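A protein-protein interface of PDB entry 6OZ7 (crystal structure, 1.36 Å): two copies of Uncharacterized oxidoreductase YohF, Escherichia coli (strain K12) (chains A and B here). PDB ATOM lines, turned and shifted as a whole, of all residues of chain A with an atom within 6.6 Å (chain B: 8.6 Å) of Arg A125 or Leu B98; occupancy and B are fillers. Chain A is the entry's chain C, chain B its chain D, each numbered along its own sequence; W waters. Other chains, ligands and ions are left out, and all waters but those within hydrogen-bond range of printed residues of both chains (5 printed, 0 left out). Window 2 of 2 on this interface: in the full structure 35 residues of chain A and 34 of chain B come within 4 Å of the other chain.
No position is printed for both chains.
Of the 12 pairs that touch across the chains among the printed residues, none has its exchanged pair printed and touching as well.
Printed residues of chain B that touch a printed residue of chain A: Pro B96, Phe B97, Leu B98, Met B100, Phe B102, Pro B149 and Asp B150.
Hydrophobic or aromatic side chains of chain B within 4 Å of the printed part of chain A: Pro B96, Phe B97, Leu B98 and Phe B102.
Printed residues of chain A that touch a printed residue of chain B: Leu A118, Ser A120, Gln A121, Ala A124, Arg A125, Glu A171 and Leu A172.
Among the printed residues, 12 pairs touch across the chains.
The side-chain amide nitrogen (NE2) of Gln A121 sits at hydrogen-bond distance from the backbone carbonyl oxygen (O) of Phe B97 (2.9 Å).
O of Met B100 is in hydrogen-bond range of NE2 of Gln A121 (2.9 Å).
The backbone carbonyl oxygen of Leu B98 lies within hydrogen-bond range of the guanidinium group of Arg A125 (2.8 Å).
N of Phe B97 is in hydrogen-bond range of OE2 of Glu A171, at 2.8 Å.
The side-chain carboxylate of Glu A171 lies close to the backbone carbonyl oxygen of Pro B149 (3.2 Å).
The backbone carbonyl oxygen (O) of Asp B150 is in hydrogen-bond range of the backbone NH (N) of Ala B95 (3.2 Å).
Among the printed residues, pairs that only touch across the chains: Glu A171 with Pro B96 (3.4 Å), Gln A121 with Leu B98 (3.6 Å), Leu A118 with Phe B102 (3.6 Å), Ala A124 with Leu B98 (3.7 Å), Glu A171 with Asp B150 (3.8 Å), Ser A120 with Phe B97 (3.9 Å) and Leu A172 with Leu B98 (3.9995 Å).
Of the printed residues of chain B, Leu A118 touches Phe B102.
Ala A124 touches just one residue of chain B: Leu B98.
Of the printed residues of chain A, Leu B98 touches Gln A121 (3.6 Å), Ala A124 (3.7 Å), Arg A125 (2.8 Å) and Leu A172 (3.9995 Å).
Printed residues of chain A within 4 Å of Pro B149: Glu A171.
The nearest printed residue of chain A that does not touch Pro B149 is Leu A172 (6.0 Å).
Water W2 lies within hydrogen-bond range of OE1 of Gln A121 (2.7 Å), O of Met B100 (2.8 Å) and N of Phe B102 (3.2 Å).
Water W5 lies within hydrogen-bond range of the backbone carbonyl oxygen of Ala B95 (2.7 Å), the side-chain carboxylate of Glu A171 (2.7 Å), the side-chain hydroxyl of Ser B152 (2.8 Å) and the backbone NH of Phe B97 (3.1 Å).
Water W4 lies within hydrogen-bond range of the side-chain carboxylate of Glu A171 (2.8 Å), the backbone NH of Leu B98 (3.0 Å) and the backbone NH of Phe B97 (3.4 Å).
Water W3 bridges OD1 of Asp B99 and NE of Arg A125.
Water W1 lies within hydrogen-bond range of the side-chain carboxylate (OE1) of Glu A171 (2.9 Å), the backbone NH (N) of Ser B152 (3.2 Å) and the backbone NH (N) of Asp B150 (3.3 Å).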
ATOM      1  N   GLU A  73     -20.944  -3.241  13.377  1.00  0.00           N
ATOM      2  CA  GLU A  73     -20.735  -2.918  14.814  1.00  0.00           C
ATOM      3  C   GLU A  73     -20.747  -4.236  15.613  1.00  0.00           C
ATOM      4  O   GLU A  73     -19.870  -4.426  16.489  1.00  0.00           O
ATOM      5  CB  GLU A  73     -21.805  -1.963  15.339  1.00  0.00           C
ATOM      6  CG  GLU A  73     -21.700  -0.563  14.781  1.00  0.00           C
ATOM      7  CD  GLU A  73     -22.650   0.458  15.413  1.00  0.00           C
ATOM      8  OE1 GLU A  73     -23.578   0.030  16.171  1.00  0.00           O
ATOM      9  OE2 GLU A  73     -22.470   1.690  15.162  1.00  0.00           O
ATOM     10  N   LEU A 118     -20.365   4.011   5.038  1.00  0.00           N
ATOM     11  CA  LEU A 118     -20.936   3.653   6.362  1.00  0.00           C
ATOM     12  C   LEU A 118     -19.987   2.708   7.099  1.00  0.00           C
ATOM     13  O   LEU A 118     -19.802   2.865   8.301  1.00  0.00           O
ATOM     14  CB  LEU A 118     -22.302   2.997   6.161  1.00  0.00           C
ATOM     15  CG  LEU A 118     -23.434   3.928   5.749  1.00  0.00           C
ATOM     16  CD1 LEU A 118     -24.652   3.121   5.349  1.00  0.00           C
ATOM     17  CD2 LEU A 118     -23.745   4.914   6.858  1.00  0.00           C
ATOM     18  N   SER A 120     -16.664   2.456   6.735  1.00  0.00           N
ATOM     19  CA  SER A 120     -15.520   3.302   7.120  1.00  0.00           C
ATOM     20  C   SER A 120     -15.863   4.128   8.357  1.00  0.00           C
ATOM     21  O   SER A 120     -14.987   4.282   9.230  1.00  0.00           O
ATOM     22  CB  SER A 120     -15.087   4.168   5.978  1.00  0.00           C
ATOM     23  OG  SER A 120     -14.590   3.382   4.902  1.00  0.00           O
ATOM     24  N   GLN A 121     -17.049   4.732   8.423  1.00  0.00           N
ATOM     25  CA  GLN A 121     -17.419   5.543   9.598  1.00  0.00           C
ATOM     26  C   GLN A 121     -17.400   4.654  10.846  1.00  0.00           C
ATOM     27  O   GLN A 121     -16.885   5.068  11.880  1.00  0.00           O
ATOM     28  CB  GLN A 121     -18.818   6.124   9.484  1.00  0.00           C
ATOM     29  CG  GLN A 121     -18.963   7.347   8.613  1.00  0.00           C
ATOM     30  CD  GLN A 121     -20.369   7.857   8.847  1.00  0.00           C
ATOM     31  OE1 GLN A 121     -21.323   7.091   8.734  1.00  0.00           O
ATOM     32  NE2 GLN A 121     -20.487   9.125   9.215  1.00  0.00           N
ATOM     33  N   ILE A 122     -18.035   3.492  10.768  1.00  0.00           N
ATOM     34  CA  ILE A 122     -18.149   2.593  11.948  1.00  0.00           C
ATOM     35  C   ILE A 122     -16.729   2.169  12.379  1.00  0.00           C
ATOM     36  O   ILE A 122     -16.408   2.175  13.563  1.00  0.00           O
ATOM     37  CB  ILE A 122     -19.073   1.421  11.609  1.00  0.00           C
ATOM     38  CG1 ILE A 122     -20.542   1.852  11.494  1.00  0.00           C
ATOM     39  CG2 ILE A 122     -18.887   0.284  12.583  1.00  0.00           C
ATOM     40  CD1 ILE A 122     -21.447   0.852  10.800  1.00  0.00           C
ATOM     41  N   ALA A 123     -15.880   1.795  11.434  1.00  0.00           N
ATOM     42  CA  ALA A 123     -14.527   1.308  11.764  1.00  0.00           C
ATOM     43  C   ALA A 123     -13.718   2.463  12.363  1.00  0.00           C
ATOM     44  O   ALA A 123     -12.998   2.260  13.345  1.00  0.00           O
ATOM     45  CB  ALA A 123     -13.867   0.757  10.540  1.00  0.00           C
ATOM     46  N   ALA A 124     -13.759   3.629  11.735  1.00  0.00           N
ATOM     47  CA  ALA A 124     -12.951   4.795  12.160  1.00  0.00           C
ATOM     48  C   ALA A 124     -13.391   5.207  13.557  1.00  0.00           C
ATOM     49  O   ALA A 124     -12.546   5.507  14.372  1.00  0.00           O
ATOM     50  CB  ALA A 124     -13.053   5.939  11.173  1.00  0.00           C
ATOM     51  N   ARG A 125     -14.684   5.201  13.850  1.00  0.00           N
ATOM     52  CA  ARG A 125     -15.138   5.544  15.219  1.00  0.00           C
ATOM     53  C   ARG A 125     -14.490   4.609  16.244  1.00  0.00           C
ATOM     54  O   ARG A 125     -14.015   5.080  17.306  1.00  0.00           O
ATOM     55  CB  ARG A 125     -16.658   5.469  15.290  1.00  0.00           C
ATOM     56  CG  ARG A 125     -17.387   6.614  14.613  1.00  0.00           C
ATOM     57  CD  ARG A 125     -18.862   6.255  14.606  1.00  0.00           C
ATOM     58  NE  ARG A 125     -19.634   7.144  13.768  1.00  0.00           N
ATOM     59  CZ  ARG A 125     -20.749   6.791  13.125  1.00  0.00           C
ATOM     60  NH1 ARG A 125     -21.224   5.560  13.232  1.00  0.00           N
ATOM     61  NH2 ARG A 125     -21.373   7.672  12.365  1.00  0.00           N
ATOM     62  N   GLN A 126     -14.470   3.318  15.961  1.00  0.00           N
ATOM     63  CA  GLN A 126     -13.897   2.328  16.891  1.00  0.00           C
ATOM     64  C   GLN A 126     -12.380   2.521  16.959  1.00  0.00           C
ATOM     65  O   GLN A 126     -11.808   2.446  18.048  1.00  0.00           O
ATOM     66  CB  GLN A 126     -14.273   0.930  16.422  1.00  0.00           C
ATOM     67  CG  GLN A 126     -13.626  -0.153  17.254  1.00  0.00           C
ATOM     68  CD  GLN A 126     -14.135  -0.215  18.670  1.00  0.00           C
ATOM     69  OE1 GLN A 126     -15.232   0.283  18.999  1.00  0.00           O
ATOM     70  NE2 GLN A 126     -13.314  -0.835  19.510  1.00  0.00           N
ATOM     71  N   MET A 127     -11.726   2.779  15.836  1.00  0.00           N
ATOM     72  CA  MET A 127     -10.280   3.025  15.875  1.00  0.00           C
ATOM     73  C   MET A 127      -9.970   4.255  16.731  1.00  0.00           C
ATOM     74  O   MET A 127      -8.989   4.250  17.484  1.00  0.00           O
ATOM     75  CB  MET A 127      -9.736   3.207  14.463  1.00  0.00           C
ATOM     76  CG  MET A 127      -9.763   1.923  13.671  1.00  0.00           C
ATOM     77  SD  MET A 127      -9.474   2.229  11.939  1.00  0.00           S
ATOM     78  CE  MET A 127      -9.658   0.563  11.303  1.00  0.00           C
ATOM     79  N   VAL A 128     -10.762   5.297  16.616  1.00  0.00           N
ATOM     80  CA  VAL A 128     -10.544   6.528  17.410  1.00  0.00           C
ATOM     81  C   VAL A 128     -10.682   6.173  18.898  1.00  0.00           C
ATOM     82  O   VAL A 128      -9.848   6.622  19.693  1.00  0.00           O
ATOM     83  CB  VAL A 128     -11.539   7.626  16.992  1.00  0.00           C
ATOM     84  CG1 VAL A 128     -11.531   8.745  18.013  1.00  0.00           C
ATOM     85  CG2 VAL A 128     -11.212   8.134  15.598  1.00  0.00           C
ATOM     86  N   LYS A 129     -11.724   5.420  19.256  1.00  0.00           N
ATOM     87  CA  LYS A 129     -11.977   5.072  20.677  1.00  0.00           C
ATOM     88  C   LYS A 129     -10.812   4.218  21.195  1.00  0.00           C
ATOM     89  O   LYS A 129     -10.391   4.428  22.337  1.00  0.00           O
ATOM     90  CB  LYS A 129     -13.327   4.374  20.864  1.00  0.00           C
ATOM     91  CG  LYS A 129     -14.570   5.231  20.648  1.00  0.00           C
ATOM     92  CD  LYS A 129     -14.827   6.318  21.675  1.00  0.00           C
ATOM     93  CE  LYS A 129     -16.228   6.885  21.563  1.00  0.00           C
ATOM     94  NZ  LYS A 129     -16.514   7.899  22.602  1.00  0.00           N
ATOM     95  N   GLN A 130     -10.305   3.300  20.399  1.00  0.00           N
ATOM     96  CA  GLN A 130      -9.153   2.448  20.825  1.00  0.00           C
ATOM     97  C   GLN A 130      -7.915   3.309  21.104  1.00  0.00           C
ATOM     98  O   GLN A 130      -7.172   2.982  22.055  1.00  0.00           O
ATOM     99  CB  GLN A 130      -8.833   1.387  19.783  1.00  0.00           C
ATOM    100  CG  GLN A 130      -9.932   0.370  19.610  1.00  0.00           C
ATOM    101  CD  GLN A 130      -9.882  -0.441  18.343  1.00  0.00           C
ATOM    102  OE1 GLN A 130     -10.729  -1.314  18.147  1.00  0.00           O
ATOM    103  NE2 GLN A 130      -8.863  -0.224  17.521  1.00  0.00           N
ATOM    104  N   GLU A 171      -8.639  13.766   7.012  1.00  0.00           N
ATOM    105  CA  GLU A 171      -9.469  14.119   8.182  1.00  0.00           C
ATOM    106  C   GLU A 171      -9.120  13.236   9.395  1.00  0.00           C
ATOM    107  O   GLU A 171      -9.282  13.737  10.529  1.00  0.00           O
ATOM    108  CB  GLU A 171     -10.933  14.008   7.791  1.00  0.00           C
ATOM    109  CG  GLU A 171     -11.848  14.529   8.842  1.00  0.00           C
ATOM    110  CD  GLU A 171     -13.237  14.887   8.364  1.00  0.00           C
ATOM    111  OE1 GLU A 171     -13.470  14.893   7.118  1.00  0.00           O
ATOM    112  OE2 GLU A 171     -14.070  15.190   9.241  1.00  0.00           O
ATOM    113  N   LEU A 172      -8.678  11.992   9.193  1.00  0.00           N
ATOM    114  CA  LEU A 172      -8.423  11.020  10.278  1.00  0.00           C
ATOM    115  C   LEU A 172      -6.936  10.970  10.657  1.00  0.00           C
ATOM    116  O   LEU A 172      -6.598  10.189  11.541  1.00  0.00           O
ATOM    117  CB  LEU A 172      -8.947   9.648   9.857  1.00  0.00           C
ATOM    118  CG  LEU A 172     -10.448   9.545   9.608  1.00  0.00           C
ATOM    119  CD1 LEU A 172     -10.777   8.145   9.141  1.00  0.00           C
ATOM    120  CD2 LEU A 172     -11.250   9.843  10.853  1.00  0.00           C
ATOM    121  N   HIS A 175      -5.480  10.886  14.191  1.00  0.00           N
ATOM    122  CA  HIS A 175      -5.788   9.618  14.905  1.00  0.00           C
ATOM    123  C   HIS A 175      -4.858   8.503  14.429  1.00  0.00           C
ATOM    124  O   HIS A 175      -5.015   7.380  14.908  1.00  0.00           O
ATOM    125  CB  HIS A 175      -7.257   9.238  14.708  1.00  0.00           C
ATOM    126  CG  HIS A 175      -8.191  10.266  15.221  1.00  0.00           C
ATOM    127  ND1 HIS A 175      -8.288  10.565  16.576  1.00  0.00           N
ATOM    128  CD2 HIS A 175      -9.053  11.083  14.576  1.00  0.00           C
ATOM    129  CE1 HIS A 175      -9.184  11.528  16.728  1.00  0.00           C
ATOM    130  NE2 HIS A 175      -9.674  11.849  15.517  1.00  0.00           N
ATOM    131  N   ILE A 177      -4.925   7.064  11.656  1.00  0.00           N
ATOM    132  CA  ILE A 177      -5.684   6.104  10.819  1.00  0.00           C
ATOM    133  C   ILE A 177      -5.238   6.354   9.392  1.00  0.00           C
ATOM    134  O   ILE A 177      -5.472   7.466   8.889  1.00  0.00           O
ATOM    135  CB  ILE A 177      -7.203   6.238  11.004  1.00  0.00           C
ATOM    136  CG1 ILE A 177      -7.602   5.953  12.450  1.00  0.00           C
ATOM    137  CG2 ILE A 177      -7.916   5.348  10.014  1.00  0.00           C
ATOM    138  CD1 ILE A 177      -9.025   6.324  12.807  1.00  0.00           C
ATOM    139  N   ALA B  95     -19.160  19.089   6.743  1.00  0.00           N
ATOM    140  CA  ALA B  95     -19.724  18.218   7.789  1.00  0.00           C
ATOM    141  C   ALA B  95     -18.651  17.227   8.179  1.00  0.00           C
ATOM    142  O   ALA B  95     -18.098  16.564   7.308  1.00  0.00           O
ATOM    143  CB  ALA B  95     -20.944  17.468   7.323  1.00  0.00           C
ATOM    144  N   PRO B  96     -18.263  17.171   9.463  1.00  0.00           N
ATOM    145  CA  PRO B  96     -17.251  16.212   9.901  1.00  0.00           C
ATOM    146  C   PRO B  96     -17.647  14.763   9.577  1.00  0.00           C
ATOM    147  O   PRO B  96     -18.803  14.334   9.675  1.00  0.00           O
ATOM    148  CB  PRO B  96     -17.132  16.477  11.408  1.00  0.00           C
ATOM    149  CG  PRO B  96     -17.677  17.866  11.592  1.00  0.00           C
ATOM    150  CD  PRO B  96     -18.741  18.045  10.537  1.00  0.00           C
ATOM    151  N   PHE B  97     -16.664  14.030   9.091  1.00  0.00           N
ATOM    152  CA  PHE B  97     -16.790  12.635   8.621  1.00  0.00           C
ATOM    153  C   PHE B  97     -17.346  11.748   9.730  1.00  0.00           C
ATOM    154  O   PHE B  97     -18.273  10.987   9.464  1.00  0.00           O
ATOM    155  CB  PHE B  97     -15.425  12.130   8.133  1.00  0.00           C
ATOM    156  CG  PHE B  97     -15.440  10.656   7.840  1.00  0.00           C
ATOM    157  CD1 PHE B  97     -16.059  10.160   6.695  1.00  0.00           C
ATOM    158  CD2 PHE B  97     -14.878   9.753   8.725  1.00  0.00           C
ATOM    159  CE1 PHE B  97     -16.133   8.795   6.471  1.00  0.00           C
ATOM    160  CE2 PHE B  97     -14.939   8.402   8.485  1.00  0.00           C
ATOM    161  CZ  PHE B  97     -15.567   7.919   7.371  1.00  0.00           C
ATOM    162  N   LEU B  98     -16.760  11.764  10.926  1.00  0.00           N
ATOM    163  CA  LEU B  98     -17.055  10.686  11.906  1.00  0.00           C
ATOM    164  C   LEU B  98     -18.545  10.709  12.275  1.00  0.00           C
ATOM    165  O   LEU B  98     -19.122   9.611  12.500  1.00  0.00           O
ATOM    166  CB  LEU B  98     -16.165  10.848  13.143  1.00  0.00           C
ATOM    167  CG  LEU B  98     -14.711  10.390  12.962  1.00  0.00           C
ATOM    168  CD1 LEU B  98     -13.847  10.842  14.136  1.00  0.00           C
ATOM    169  CD2 LEU B  98     -14.610   8.870  12.792  1.00  0.00           C
ATOM    170  N   ASP B  99     -19.152  11.901  12.289  1.00  0.00           N
ATOM    171  CA  ASP B  99     -20.538  12.021  12.816  1.00  0.00           C
ATOM    172  C   ASP B  99     -21.554  12.357  11.721  1.00  0.00           C
ATOM    173  O   ASP B  99     -22.751  12.503  12.038  1.00  0.00           O
ATOM    174  CB  ASP B  99     -20.635  13.055  13.946  1.00  0.00           C
ATOM    175  CG  ASP B  99     -19.992  12.618  15.251  1.00  0.00           C
ATOM    176  OD1 ASP B  99     -20.527  11.688  15.881  1.00  0.00           O
ATOM    177  OD2 ASP B  99     -18.943  13.202  15.616  1.00  0.00           O
ATOM    178  N   MET B 100     -21.158  12.389  10.460  1.00  0.00           N
ATOM    179  CA  MET B 100     -22.100  12.786   9.384  1.00  0.00           C
ATOM    180  C   MET B 100     -23.267  11.791   9.301  1.00  0.00           C
ATOM    181  O   MET B 100     -23.046  10.576   9.201  1.00  0.00           O
ATOM    182  CB  MET B 100     -21.387  12.865   8.037  1.00  0.00           C
ATOM    183  CG  MET B 100     -22.261  13.452   6.974  1.00  0.00           C
ATOM    184  SD  MET B 100     -21.418  13.627   5.422  1.00  0.00           S
ATOM    185  CE  MET B 100     -22.268  15.094   4.832  1.00  0.00           C
ATOM    186  N   ALA B 101     -24.488  12.308   9.323  1.00  0.00           N
ATOM    187  CA  ALA B 101     -25.702  11.486   9.128  1.00  0.00           C
ATOM    188  C   ALA B 101     -25.723  10.963   7.691  1.00  0.00           C
ATOM    189  O   ALA B 101     -25.265  11.665   6.757  1.00  0.00           O
ATOM    190  CB  ALA B 101     -26.934  12.294   9.434  1.00  0.00           C
ATOM    191  N   PHE B 102     -26.303   9.791   7.495  1.00  0.00           N
ATOM    192  CA  PHE B 102     -26.328   9.157   6.164  1.00  0.00           C
ATOM    193  C   PHE B 102     -27.154  10.032   5.222  1.00  0.00           C
ATOM    194  O   PHE B 102     -26.804  10.153   4.032  1.00  0.00           O
ATOM    195  CB  PHE B 102     -26.861   7.735   6.254  1.00  0.00           C
ATOM    196  CG  PHE B 102     -26.753   6.970   4.963  1.00  0.00           C
ATOM    197  CD1 PHE B 102     -25.541   6.805   4.321  1.00  0.00           C
ATOM    198  CD2 PHE B 102     -27.862   6.355   4.422  1.00  0.00           C
ATOM    199  CE1 PHE B 102     -25.470   6.108   3.126  1.00  0.00           C
ATOM    200  CE2 PHE B 102     -27.776   5.638   3.246  1.00  0.00           C
ATOM    201  CZ  PHE B 102     -26.572   5.479   2.620  1.00  0.00           C
ATOM    202  N   PRO B 149     -10.265  18.851   4.448  1.00  0.00           N
ATOM    203  CA  PRO B 149     -10.070  18.092   5.690  1.00  0.00           C
ATOM    204  C   PRO B 149     -11.346  17.887   6.528  1.00  0.00           C
ATOM    205  O   PRO B 149     -11.241  17.192   7.526  1.00  0.00           O
ATOM    206  CB  PRO B 149      -9.052  18.986   6.424  1.00  0.00           C
ATOM    207  CG  PRO B 149      -9.501  20.399   6.047  1.00  0.00           C
ATOM    208  CD  PRO B 149      -9.874  20.264   4.585  1.00  0.00           C
ATOM    209  N   ASP B 150     -12.482  18.458   6.085  1.00  0.00           N
ATOM    210  CA  ASP B 150     -13.748  18.636   6.855  1.00  0.00           C
ATOM    211  C   ASP B 150     -14.964  18.634   5.919  1.00  0.00           C
ATOM    212  O   ASP B 150     -16.016  19.084   6.282  1.00  0.00           O
ATOM    213  CB  ASP B 150     -13.681  19.934   7.657  1.00  0.00           C
ATOM    214  CG  ASP B 150     -13.318  21.134   6.791  1.00  0.00           C
ATOM    215  OD1 ASP B 150     -13.020  20.954   5.555  1.00  0.00           O
ATOM    216  OD2 ASP B 150     -13.308  22.245   7.369  1.00  0.00           O
ATOM    217  N   SER B 152     -15.872  15.653   3.482  1.00  0.00           N
ATOM    218  CA  SER B 152     -15.622  14.361   2.804  1.00  0.00           C
ATOM    219  C   SER B 152     -16.711  14.075   1.762  1.00  0.00           C
ATOM    220  O   SER B 152     -16.371  13.598   0.656  1.00  0.00           O
ATOM    221  CB  SER B 152     -15.483  13.264   3.802  1.00  0.00           C
ATOM    222  OG  SER B 152     -16.648  13.046   4.584  1.00  0.00           O
HETATM  223  O   HOH W   1     -12.800  15.658   4.402  1.00  0.00           O
HETATM  224  O   HOH W   2     -23.829   7.982   8.477  1.00  0.00           O
HETATM  225  O   HOH W   3     -19.025   9.257  16.089  1.00  0.00           O
HETATM  226  O   HOH W   4     -14.312  13.480  11.451  1.00  0.00           O
HETATM  227  O   HOH W   5     -16.016  15.197   6.282  1.00  0.00           O
